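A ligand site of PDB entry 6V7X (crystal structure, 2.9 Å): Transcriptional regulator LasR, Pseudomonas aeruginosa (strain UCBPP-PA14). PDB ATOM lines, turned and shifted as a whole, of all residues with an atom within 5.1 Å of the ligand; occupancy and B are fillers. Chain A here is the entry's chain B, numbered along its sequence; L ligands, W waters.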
ATOM      1  N   LEU A  36     -13.059   6.291 -26.685  1.00  0.00           N
ATOM      2  CA  LEU A  36     -11.675   6.266 -27.134  1.00  0.00           C
ATOM      3  C   LEU A  36     -10.868   5.398 -26.181  1.00  0.00           C
ATOM      4  O   LEU A  36     -11.010   5.513 -24.967  1.00  0.00           O
ATOM      5  CB  LEU A  36     -11.078   7.685 -27.195  1.00  0.00           C
ATOM      6  CG  LEU A  36      -9.578   7.784 -27.511  1.00  0.00           C
ATOM      7  CD1 LEU A  36      -9.330   8.917 -28.483  1.00  0.00           C
ATOM      8  CD2 LEU A  36      -8.748   7.973 -26.241  1.00  0.00           C
ATOM      9  N   GLY A  38      -6.944   4.640 -25.579  1.00  0.00           N
ATOM     10  CA  GLY A  38      -5.549   4.937 -25.854  1.00  0.00           C
ATOM     11  C   GLY A  38      -4.656   4.102 -24.959  1.00  0.00           C
ATOM     12  O   GLY A  38      -5.009   3.775 -23.826  1.00  0.00           O
ATOM     13  N   LEU A  39      -3.484   3.727 -25.489  1.00  0.00           N
ATOM     14  CA  LEU A  39      -2.526   2.958 -24.716  1.00  0.00           C
ATOM     15  C   LEU A  39      -1.127   3.251 -25.229  1.00  0.00           C
ATOM     16  O   LEU A  39      -0.929   3.499 -26.422  1.00  0.00           O
ATOM     17  CB  LEU A  39      -2.809   1.452 -24.793  1.00  0.00           C
ATOM     18  CG  LEU A  39      -2.216   0.596 -23.666  1.00  0.00           C
ATOM     19  CD1 LEU A  39      -2.271   1.322 -22.331  1.00  0.00           C
ATOM     20  CD2 LEU A  39      -2.902  -0.761 -23.584  1.00  0.00           C
ATOM     21  N   LEU A  40      -0.161   3.205 -24.315  1.00  0.00           N
ATOM     22  CA  LEU A  40       1.230   3.435 -24.642  1.00  0.00           C
ATOM     23  C   LEU A  40       2.087   2.335 -24.038  1.00  0.00           C
ATOM     24  O   LEU A  40       1.699   1.723 -23.039  1.00  0.00           O
ATOM     25  CB  LEU A  40       1.702   4.798 -24.137  1.00  0.00           C
ATOM     26  CG  LEU A  40       1.475   5.965 -25.081  1.00  0.00           C
ATOM     27  CD1 LEU A  40       1.737   7.281 -24.375  1.00  0.00           C
ATOM     28  CD2 LEU A  40       2.377   5.833 -26.298  1.00  0.00           C
ATOM     29  N   TYR A  47       2.914  10.981 -26.507  1.00  0.00           N
ATOM     30  CA  TYR A  47       1.552  10.567 -26.772  1.00  0.00           C
ATOM     31  C   TYR A  47       1.227  10.479 -28.257  1.00  0.00           C
ATOM     32  O   TYR A  47       0.212   9.857 -28.622  1.00  0.00           O
ATOM     33  CB  TYR A  47       0.574  11.511 -26.073  1.00  0.00           C
ATOM     34  CG  TYR A  47       1.014  11.869 -24.683  1.00  0.00           C
ATOM     35  CD1 TYR A  47       1.015  10.912 -23.678  1.00  0.00           C
ATOM     36  CD2 TYR A  47       1.442  13.153 -24.372  1.00  0.00           C
ATOM     37  CE1 TYR A  47       1.415  11.232 -22.402  1.00  0.00           C
ATOM     38  CE2 TYR A  47       1.850  13.468 -23.094  1.00  0.00           C
ATOM     39  CZ  TYR A  47       1.831  12.505 -22.118  1.00  0.00           C
ATOM     40  OH  TYR A  47       2.239  12.820 -20.840  1.00  0.00           O
ATOM     41  N   ALA A  50       0.738   6.613 -30.576  1.00  0.00           N
ATOM     42  CA  ALA A  50       0.197   5.703 -29.580  1.00  0.00           C
ATOM     43  C   ALA A  50      -0.875   4.800 -30.200  1.00  0.00           C
ATOM     44  O   ALA A  50      -1.369   5.060 -31.301  1.00  0.00           O
ATOM     45  CB  ALA A  50      -0.405   6.478 -28.400  1.00  0.00           C
ATOM     46  N   ILE A  52      -4.324   4.077 -30.489  1.00  0.00           N
ATOM     47  CA  ILE A  52      -5.553   4.836 -30.261  1.00  0.00           C
ATOM     48  C   ILE A  52      -6.610   4.350 -31.237  1.00  0.00           C
ATOM     49  O   ILE A  52      -6.458   4.496 -32.455  1.00  0.00           O
ATOM     50  CB  ILE A  52      -5.335   6.356 -30.437  1.00  0.00           C
ATOM     51  CG1 ILE A  52      -4.263   6.874 -29.483  1.00  0.00           C
ATOM     52  CG2 ILE A  52      -6.630   7.104 -30.217  1.00  0.00           C
ATOM     53  CD1 ILE A  52      -3.816   8.311 -29.789  1.00  0.00           C
ATOM     54  N   TYR A  56     -14.296   8.097 -31.861  1.00  0.00           N
ATOM     55  CA  TYR A  56     -14.278   9.550 -31.871  1.00  0.00           C
ATOM     56  C   TYR A  56     -14.360  10.033 -33.313  1.00  0.00           C
ATOM     57  O   TYR A  56     -13.818   9.387 -34.210  1.00  0.00           O
ATOM     58  CB  TYR A  56     -13.003  10.085 -31.206  1.00  0.00           C
ATOM     59  CG  TYR A  56     -13.092  10.298 -29.702  1.00  0.00           C
ATOM     60  CD1 TYR A  56     -14.154   9.817 -28.954  1.00  0.00           C
ATOM     61  CD2 TYR A  56     -12.075  10.984 -29.031  1.00  0.00           C
ATOM     62  CE1 TYR A  56     -14.216  10.012 -27.586  1.00  0.00           C
ATOM     63  CE2 TYR A  56     -12.138  11.179 -27.662  1.00  0.00           C
ATOM     64  CZ  TYR A  56     -13.206  10.693 -26.946  1.00  0.00           C
ATOM     65  OH  TYR A  56     -13.247  10.901 -25.577  1.00  0.00           O
ATOM     66  N   TRP A  60     -12.072  15.129 -35.595  1.00  0.00           N
ATOM     67  CA  TRP A  60     -11.539  15.582 -34.315  1.00  0.00           C
ATOM     68  C   TRP A  60     -10.262  14.822 -33.949  1.00  0.00           C
ATOM     69  O   TRP A  60      -9.324  15.410 -33.395  1.00  0.00           O
ATOM     70  CB  TRP A  60     -12.593  15.406 -33.215  1.00  0.00           C
ATOM     71  CG  TRP A  60     -12.054  15.580 -31.814  1.00  0.00           C
ATOM     72  CD1 TRP A  60     -11.857  14.609 -30.885  1.00  0.00           C
ATOM     73  CD2 TRP A  60     -11.658  16.820 -31.195  1.00  0.00           C
ATOM     74  NE1 TRP A  60     -11.356  15.148 -29.728  1.00  0.00           N
ATOM     75  CE2 TRP A  60     -11.221  16.504 -29.894  1.00  0.00           C
ATOM     76  CE3 TRP A  60     -11.627  18.147 -31.617  1.00  0.00           C
ATOM     77  CZ2 TRP A  60     -10.769  17.478 -29.001  1.00  0.00           C
ATOM     78  CZ3 TRP A  60     -11.167  19.110 -30.730  1.00  0.00           C
ATOM     79  CH2 TRP A  60     -10.744  18.770 -29.436  1.00  0.00           C
ATOM     80  N   ARG A  61     -10.220  13.519 -34.235  1.00  0.00           N
ATOM     81  CA  ARG A  61      -9.037  12.720 -33.927  1.00  0.00           C
ATOM     82  C   ARG A  61      -7.818  13.237 -34.671  1.00  0.00           C
ATOM     83  O   ARG A  61      -6.749  13.434 -34.084  1.00  0.00           O
ATOM     84  CB  ARG A  61      -9.302  11.254 -34.273  1.00  0.00           C
ATOM     85  CG  ARG A  61     -10.152  10.520 -33.256  1.00  0.00           C
ATOM     86  CD  ARG A  61      -9.369  10.235 -31.984  1.00  0.00           C
ATOM     87  NE  ARG A  61      -7.953   9.994 -32.260  1.00  0.00           N
ATOM     88  CZ  ARG A  61      -6.958  10.698 -31.729  1.00  0.00           C
ATOM     89  NH1 ARG A  61      -7.221  11.690 -30.901  1.00  0.00           N
ATOM     90  NH2 ARG A  61      -5.695  10.411 -32.040  1.00  0.00           N
ATOM     91  N   TYR A  64      -6.791  16.481 -33.143  1.00  0.00           N
ATOM     92  CA  TYR A  64      -6.204  16.315 -31.815  1.00  0.00           C
ATOM     93  C   TYR A  64      -4.716  16.005 -31.900  1.00  0.00           C
ATOM     94  O   TYR A  64      -3.929  16.465 -31.065  1.00  0.00           O
ATOM     95  CB  TYR A  64      -6.955  15.211 -31.074  1.00  0.00           C
ATOM     96  CG  TYR A  64      -6.554  15.017 -29.632  1.00  0.00           C
ATOM     97  CD1 TYR A  64      -7.350  15.499 -28.597  1.00  0.00           C
ATOM     98  CD2 TYR A  64      -5.390  14.336 -29.291  1.00  0.00           C
ATOM     99  CE1 TYR A  64      -6.995  15.314 -27.275  1.00  0.00           C
ATOM    100  CE2 TYR A  64      -5.026  14.145 -27.967  1.00  0.00           C
ATOM    101  CZ  TYR A  64      -5.831  14.635 -26.971  1.00  0.00           C
ATOM    102  OH  TYR A  64      -5.476  14.444 -25.657  1.00  0.00           O
ATOM    103  N   ALA A  70      -2.476  16.392 -26.730  1.00  0.00           N
ATOM    104  CA  ALA A  70      -2.195  15.471 -25.640  1.00  0.00           C
ATOM    105  C   ALA A  70      -1.464  16.157 -24.488  1.00  0.00           C
ATOM    106  O   ALA A  70      -1.617  15.753 -23.331  1.00  0.00           O
ATOM    107  CB  ALA A  70      -1.379  14.299 -26.158  1.00  0.00           C
ATOM    108  N   ASP A  73      -4.554  18.546 -22.959  1.00  0.00           N
ATOM    109  CA  ASP A  73      -5.743  17.855 -22.490  1.00  0.00           C
ATOM    110  C   ASP A  73      -5.633  17.558 -20.992  1.00  0.00           C
ATOM    111  O   ASP A  73      -4.685  16.883 -20.567  1.00  0.00           O
ATOM    112  CB  ASP A  73      -5.939  16.554 -23.263  1.00  0.00           C
ATOM    113  CG  ASP A  73      -7.338  15.985 -23.110  1.00  0.00           C
ATOM    114  OD1 ASP A  73      -7.957  16.185 -22.046  1.00  0.00           O
ATOM    115  OD2 ASP A  73      -7.815  15.332 -24.052  1.00  0.00           O
ATOM    116  N   THR A  75      -7.226  15.507 -19.264  1.00  0.00           N
ATOM    117  CA  THR A  75      -7.545  14.126 -18.939  1.00  0.00           C
ATOM    118  C   THR A  75      -6.313  13.239 -18.952  1.00  0.00           C
ATOM    119  O   THR A  75      -6.076  12.463 -18.022  1.00  0.00           O
ATOM    120  CB  THR A  75      -8.592  13.595 -19.923  1.00  0.00           C
ATOM    121  OG1 THR A  75      -8.044  13.625 -21.247  1.00  0.00           O
ATOM    122  CG2 THR A  75      -9.843  14.449 -19.874  1.00  0.00           C
ATOM    123  N   VAL A  76      -5.489  13.346 -20.002  1.00  0.00           N
ATOM    124  CA  VAL A  76      -4.303  12.511 -20.079  1.00  0.00           C
ATOM    125  C   VAL A  76      -3.241  12.974 -19.088  1.00  0.00           C
ATOM    126  O   VAL A  76      -2.513  12.150 -18.527  1.00  0.00           O
ATOM    127  CB  VAL A  76      -3.774  12.472 -21.536  1.00  0.00           C
ATOM    128  CG1 VAL A  76      -3.696  13.863 -22.102  1.00  0.00           C
ATOM    129  CG2 VAL A  76      -2.417  11.778 -21.595  1.00  0.00           C
ATOM    130  N   CYS A  79      -4.250  11.056 -16.083  1.00  0.00           N
ATOM    131  CA  CYS A  79      -3.923   9.630 -16.147  1.00  0.00           C
ATOM    132  C   CYS A  79      -2.456   9.326 -15.848  1.00  0.00           C
ATOM    133  O   CYS A  79      -2.154   8.166 -15.530  1.00  0.00           O
ATOM    134  CB  CYS A  79      -4.253   9.019 -17.506  1.00  0.00           C
ATOM    135  SG  CYS A  79      -5.959   9.147 -18.127  1.00  0.00           S
ATOM    136  N   TRP A  88     -15.423  15.346 -17.057  1.00  0.00           N
ATOM    137  CA  TRP A  88     -15.173  16.500 -17.898  1.00  0.00           C
ATOM    138  C   TRP A  88     -15.990  17.699 -17.445  1.00  0.00           C
ATOM    139  O   TRP A  88     -16.750  18.277 -18.227  1.00  0.00           O
ATOM    140  CB  TRP A  88     -15.463  16.171 -19.362  1.00  0.00           C
ATOM    141  CG  TRP A  88     -14.731  14.956 -19.854  1.00  0.00           C
ATOM    142  CD1 TRP A  88     -13.710  14.298 -19.222  1.00  0.00           C
ATOM    143  CD2 TRP A  88     -14.967  14.251 -21.069  1.00  0.00           C
ATOM    144  NE1 TRP A  88     -13.302  13.221 -19.978  1.00  0.00           N
ATOM    145  CE2 TRP A  88     -14.056  13.170 -21.119  1.00  0.00           C
ATOM    146  CE3 TRP A  88     -15.864  14.416 -22.128  1.00  0.00           C
ATOM    147  CZ2 TRP A  88     -14.019  12.277 -22.174  1.00  0.00           C
ATOM    148  CZ3 TRP A  88     -15.826  13.527 -23.175  1.00  0.00           C
ATOM    149  CH2 TRP A  88     -14.911  12.468 -23.192  1.00  0.00           C
ATOM    150  N   TYR A  93     -10.631  22.504 -16.993  1.00  0.00           N
ATOM    151  CA  TYR A  93     -10.054  23.394 -17.993  1.00  0.00           C
ATOM    152  C   TYR A  93      -9.719  24.719 -17.313  1.00  0.00           C
ATOM    153  O   TYR A  93     -10.610  25.540 -17.060  1.00  0.00           O
ATOM    154  CB  TYR A  93     -11.003  23.601 -19.157  1.00  0.00           C
ATOM    155  CG  TYR A  93     -11.588  22.317 -19.687  1.00  0.00           C
ATOM    156  CD1 TYR A  93     -10.820  21.451 -20.458  1.00  0.00           C
ATOM    157  CD2 TYR A  93     -12.897  21.963 -19.410  1.00  0.00           C
ATOM    158  CE1 TYR A  93     -11.347  20.262 -20.938  1.00  0.00           C
ATOM    159  CE2 TYR A  93     -13.431  20.785 -19.884  1.00  0.00           C
ATOM    160  CZ  TYR A  93     -12.656  19.931 -20.652  1.00  0.00           C
ATOM    161  OH  TYR A  93     -13.190  18.752 -21.125  1.00  0.00           O
ATOM    162  N   PHE A 101      -9.186  24.427 -25.993  1.00  0.00           N
ATOM    163  CA  PHE A 101      -9.313  22.989 -26.206  1.00  0.00           C
ATOM    164  C   PHE A 101     -10.736  22.526 -25.904  1.00  0.00           C
ATOM    165  O   PHE A 101     -11.301  21.726 -26.655  1.00  0.00           O
ATOM    166  CB  PHE A 101      -8.309  22.241 -25.333  1.00  0.00           C
ATOM    167  CG  PHE A 101      -8.630  20.782 -25.173  1.00  0.00           C
ATOM    168  CD1 PHE A 101      -8.371  19.883 -26.204  1.00  0.00           C
ATOM    169  CD2 PHE A 101      -9.201  20.301 -24.008  1.00  0.00           C
ATOM    170  CE1 PHE A 101      -8.658  18.545 -26.066  1.00  0.00           C
ATOM    171  CE2 PHE A 101      -9.507  18.955 -23.862  1.00  0.00           C
ATOM    172  CZ  PHE A 101      -9.231  18.081 -24.901  1.00  0.00           C
ATOM    173  N   ALA A 105     -13.531  20.776 -28.367  1.00  0.00           N
ATOM    174  CA  ALA A 105     -13.988  19.417 -28.110  1.00  0.00           C
ATOM    175  C   ALA A 105     -15.510  19.341 -28.130  1.00  0.00           C
ATOM    176  O   ALA A 105     -16.090  18.336 -28.566  1.00  0.00           O
ATOM    177  CB  ALA A 105     -13.441  18.928 -26.771  1.00  0.00           C
ATOM    178  N   LEU A 110     -18.197  16.433 -27.948  1.00  0.00           N
ATOM    179  CA  LEU A 110     -17.651  15.796 -26.765  1.00  0.00           C
ATOM    180  C   LEU A 110     -17.802  16.699 -25.546  1.00  0.00           C
ATOM    181  O   LEU A 110     -16.803  17.116 -24.949  1.00  0.00           O
ATOM    182  CB  LEU A 110     -16.182  15.439 -26.973  1.00  0.00           C
ATOM    183  CG  LEU A 110     -15.813  14.474 -28.108  1.00  0.00           C
ATOM    184  CD1 LEU A 110     -14.544  13.719 -27.745  1.00  0.00           C
ATOM    185  CD2 LEU A 110     -16.951  13.488 -28.390  1.00  0.00           C
ATOM    186  N   THR A 115     -13.084  10.109 -18.116  1.00  0.00           N
ATOM    187  CA  THR A 115     -11.887   9.412 -18.560  1.00  0.00           C
ATOM    188  C   THR A 115     -11.378   8.520 -17.435  1.00  0.00           C
ATOM    189  O   THR A 115     -11.207   8.991 -16.300  1.00  0.00           O
ATOM    190  CB  THR A 115     -10.788  10.405 -18.974  1.00  0.00           C
ATOM    191  OG1 THR A 115     -11.241  11.180 -20.091  1.00  0.00           O
ATOM    192  CG2 THR A 115      -9.514   9.675 -19.334  1.00  0.00           C
ATOM    193  N   LEU A 125       0.511   2.471 -20.051  1.00  0.00           N
ATOM    194  CA  LEU A 125      -0.188   3.670 -19.625  1.00  0.00           C
ATOM    195  C   LEU A 125      -1.117   4.120 -20.746  1.00  0.00           C
ATOM    196  O   LEU A 125      -0.677   4.270 -21.895  1.00  0.00           O
ATOM    197  CB  LEU A 125       0.785   4.800 -19.260  1.00  0.00           C
ATOM    198  CG  LEU A 125       0.231   6.218 -19.402  1.00  0.00           C
ATOM    199  CD1 LEU A 125      -0.719   6.565 -18.259  1.00  0.00           C
ATOM    200  CD2 LEU A 125       1.371   7.188 -19.459  1.00  0.00           C
ATOM    201  N   GLY A 126      -2.381   4.319 -20.413  1.00  0.00           N
ATOM    202  CA  GLY A 126      -3.354   4.740 -21.402  1.00  0.00           C
ATOM    203  C   GLY A 126      -4.588   5.293 -20.728  1.00  0.00           C
ATOM    204  O   GLY A 126      -4.649   5.426 -19.499  1.00  0.00           O
ATOM    205  N   ALA A 127      -5.578   5.627 -21.550  1.00  0.00           N
ATOM    206  CA  ALA A 127      -6.832   6.208 -21.083  1.00  0.00           C
ATOM    207  C   ALA A 127      -8.008   5.545 -21.785  1.00  0.00           C
ATOM    208  O   ALA A 127      -7.900   5.133 -22.947  1.00  0.00           O
ATOM    209  CB  ALA A 127      -6.865   7.723 -21.331  1.00  0.00           C
ATOM    210  N   SER A 129     -11.802   6.807 -22.396  1.00  0.00           N
ATOM    211  CA  SER A 129     -12.730   7.919 -22.304  1.00  0.00           C
ATOM    212  C   SER A 129     -14.059   7.541 -22.944  1.00  0.00           C
ATOM    213  O   SER A 129     -14.089   6.933 -24.020  1.00  0.00           O
ATOM    214  CB  SER A 129     -12.172   9.161 -23.002  1.00  0.00           C
ATOM    215  OG  SER A 129     -11.058   9.681 -22.319  1.00  0.00           O
HETATM  216  C1  LIG L   1      -2.550   8.249 -21.181  1.00  0.00           C
HETATM  217  C2  LIG L   1      -1.904   8.273 -22.562  1.00  0.00           C
HETATM  218  C3  LIG L   1      -2.806   7.587 -23.585  1.00  0.00           C
HETATM  219  C4  LIG L   1      -2.334   7.935 -24.998  1.00  0.00           C
HETATM  220  C5  LIG L   1      -2.367   9.445 -25.171  1.00  0.00           C
HETATM  221  C6  LIG L   1      -3.214   9.827 -26.390  1.00  0.00           C
HETATM  222  C7  LIG L   1      -4.593   9.193 -26.281  1.00  0.00           C
HETATM  223  C8  LIG L   1      -5.643  10.166 -26.791  1.00  0.00           C
HETATM  224  C9  LIG L   1      -5.828  11.275 -25.761  1.00  0.00           C
HETATM  225  C10 LIG L   1      -7.310  11.615 -25.588  1.00  0.00           C
HETATM  226  O1  LIG L   1      -8.053  11.534 -26.496  1.00  0.00           O
HETATM  227  C11 LIG L   1      -7.821  12.044 -24.219  1.00  0.00           C
HETATM  228  C12 LIG L   1      -9.314  12.361 -24.270  1.00  0.00           C
HETATM  229  O2  LIG L   1     -10.106  11.502 -24.114  1.00  0.00           O
HETATM  230  N1  LIG L   1      -9.770  13.723 -24.496  1.00  0.00           N
HETATM  231  C13 LIG L   1     -11.227  14.013 -24.522  1.00  0.00           C
HETATM  232  C14 LIG L   1     -11.592  14.401 -23.241  1.00  0.00           C
HETATM  233  C15 LIG L   1     -12.331  15.818 -23.335  1.00  0.00           C
HETATM  234  C16 LIG L   1     -11.561  15.210 -25.449  1.00  0.00           C
HETATM  235  O3  LIG L   1     -11.187  15.369 -26.559  1.00  0.00           O
HETATM  236  O4  LIG L   1     -12.451  16.129 -24.685  1.00  0.00           O
HETATM  237  O   HOH W   1      -9.023  12.344 -28.793  1.00  0.00           O
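OG of Ser 129 is in hydrogen-bond range of O2 of the ligand (2.7 Å).
An oxygen (O3) of the ligand sits at hydrogen-bond distance from the indole nitrogen (NE1) of Trp 60 (3.2 Å).
The side-chain carboxylate (OD2) of Asp 73 is in hydrogen-bond range of a nitrogen (N1) of the ligand.
The backbone carbonyl oxygen of Ala 105 sits at hydrogen-bond distance from the backbone NH of Leu 110.
OG of Ser 129 sits at hydrogen-bond distance from OG1 of Thr 115 (2.7 Å).
The backbone carbonyl oxygen (O) of Leu 125 is in hydrogen-bond range of the backbone NH (N) of Leu 40 (2.7 Å).
NE1 of Trp 88 is in hydrogen-bond range of OG1 of Thr 115.
OD1 of Asp 73 sits at hydrogen-bond distance from OG1 of Thr 75 (2.7 Å).
The backbone NH of Gly 38 is in hydrogen-bond range of the backbone carbonyl oxygen of Ala 127 (2.8 Å).
OH of Tyr 64 lies within hydrogen-bond range of OD2 of Asp 73, at 3.0 Å.
O of Ser 129 sits at hydrogen-bond distance from N of Leu 36 (2.9 Å).
Residues that only touch the ligand: Leu 36 (3.5 Å), Tyr 47 (3.7 Å), Ile 52 (3.7 Å), Tyr 56 (3.5 Å), Tyr 64 (3.2 Å), Thr 75 (3.4 Å), Val 76 (3.6 Å), Trp 88 (3.4 Å), Tyr 93 (3.8 Å), Phe 101 (3.7 Å), Ala 105 (3.6 Å), Leu 110 (3.9 Å), Leu 125 (3.8 Å), Gly 126 (3.6 Å) and Ala 127 (3.96 Å).
Hydrophobic or aromatic side chains within 4 Å of the ligand: Leu 36, Tyr 47, Ile 52, Trp 60, Tyr 64, Val 76, Trp 88, Phe 101, Ala 105, Leu 110 and Leu 125.
18 residues have an atom within 4 Å of the ligand: Leu 36, Tyr 47, Ile 52, Tyr 56, Trp 60, Tyr 64, Asp 73, Thr 75, Val 76, Trp 88, Tyr 93, Phe 101, Ala 105, Leu 110, Leu 125, Gly 126, Ala 127 and Ser 129.
The nearest printed residue that does not touch the ligand is Cys 79 (4.1 Å).
Water W1 bridges O1 of the ligand and NH1 of Arg 61.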
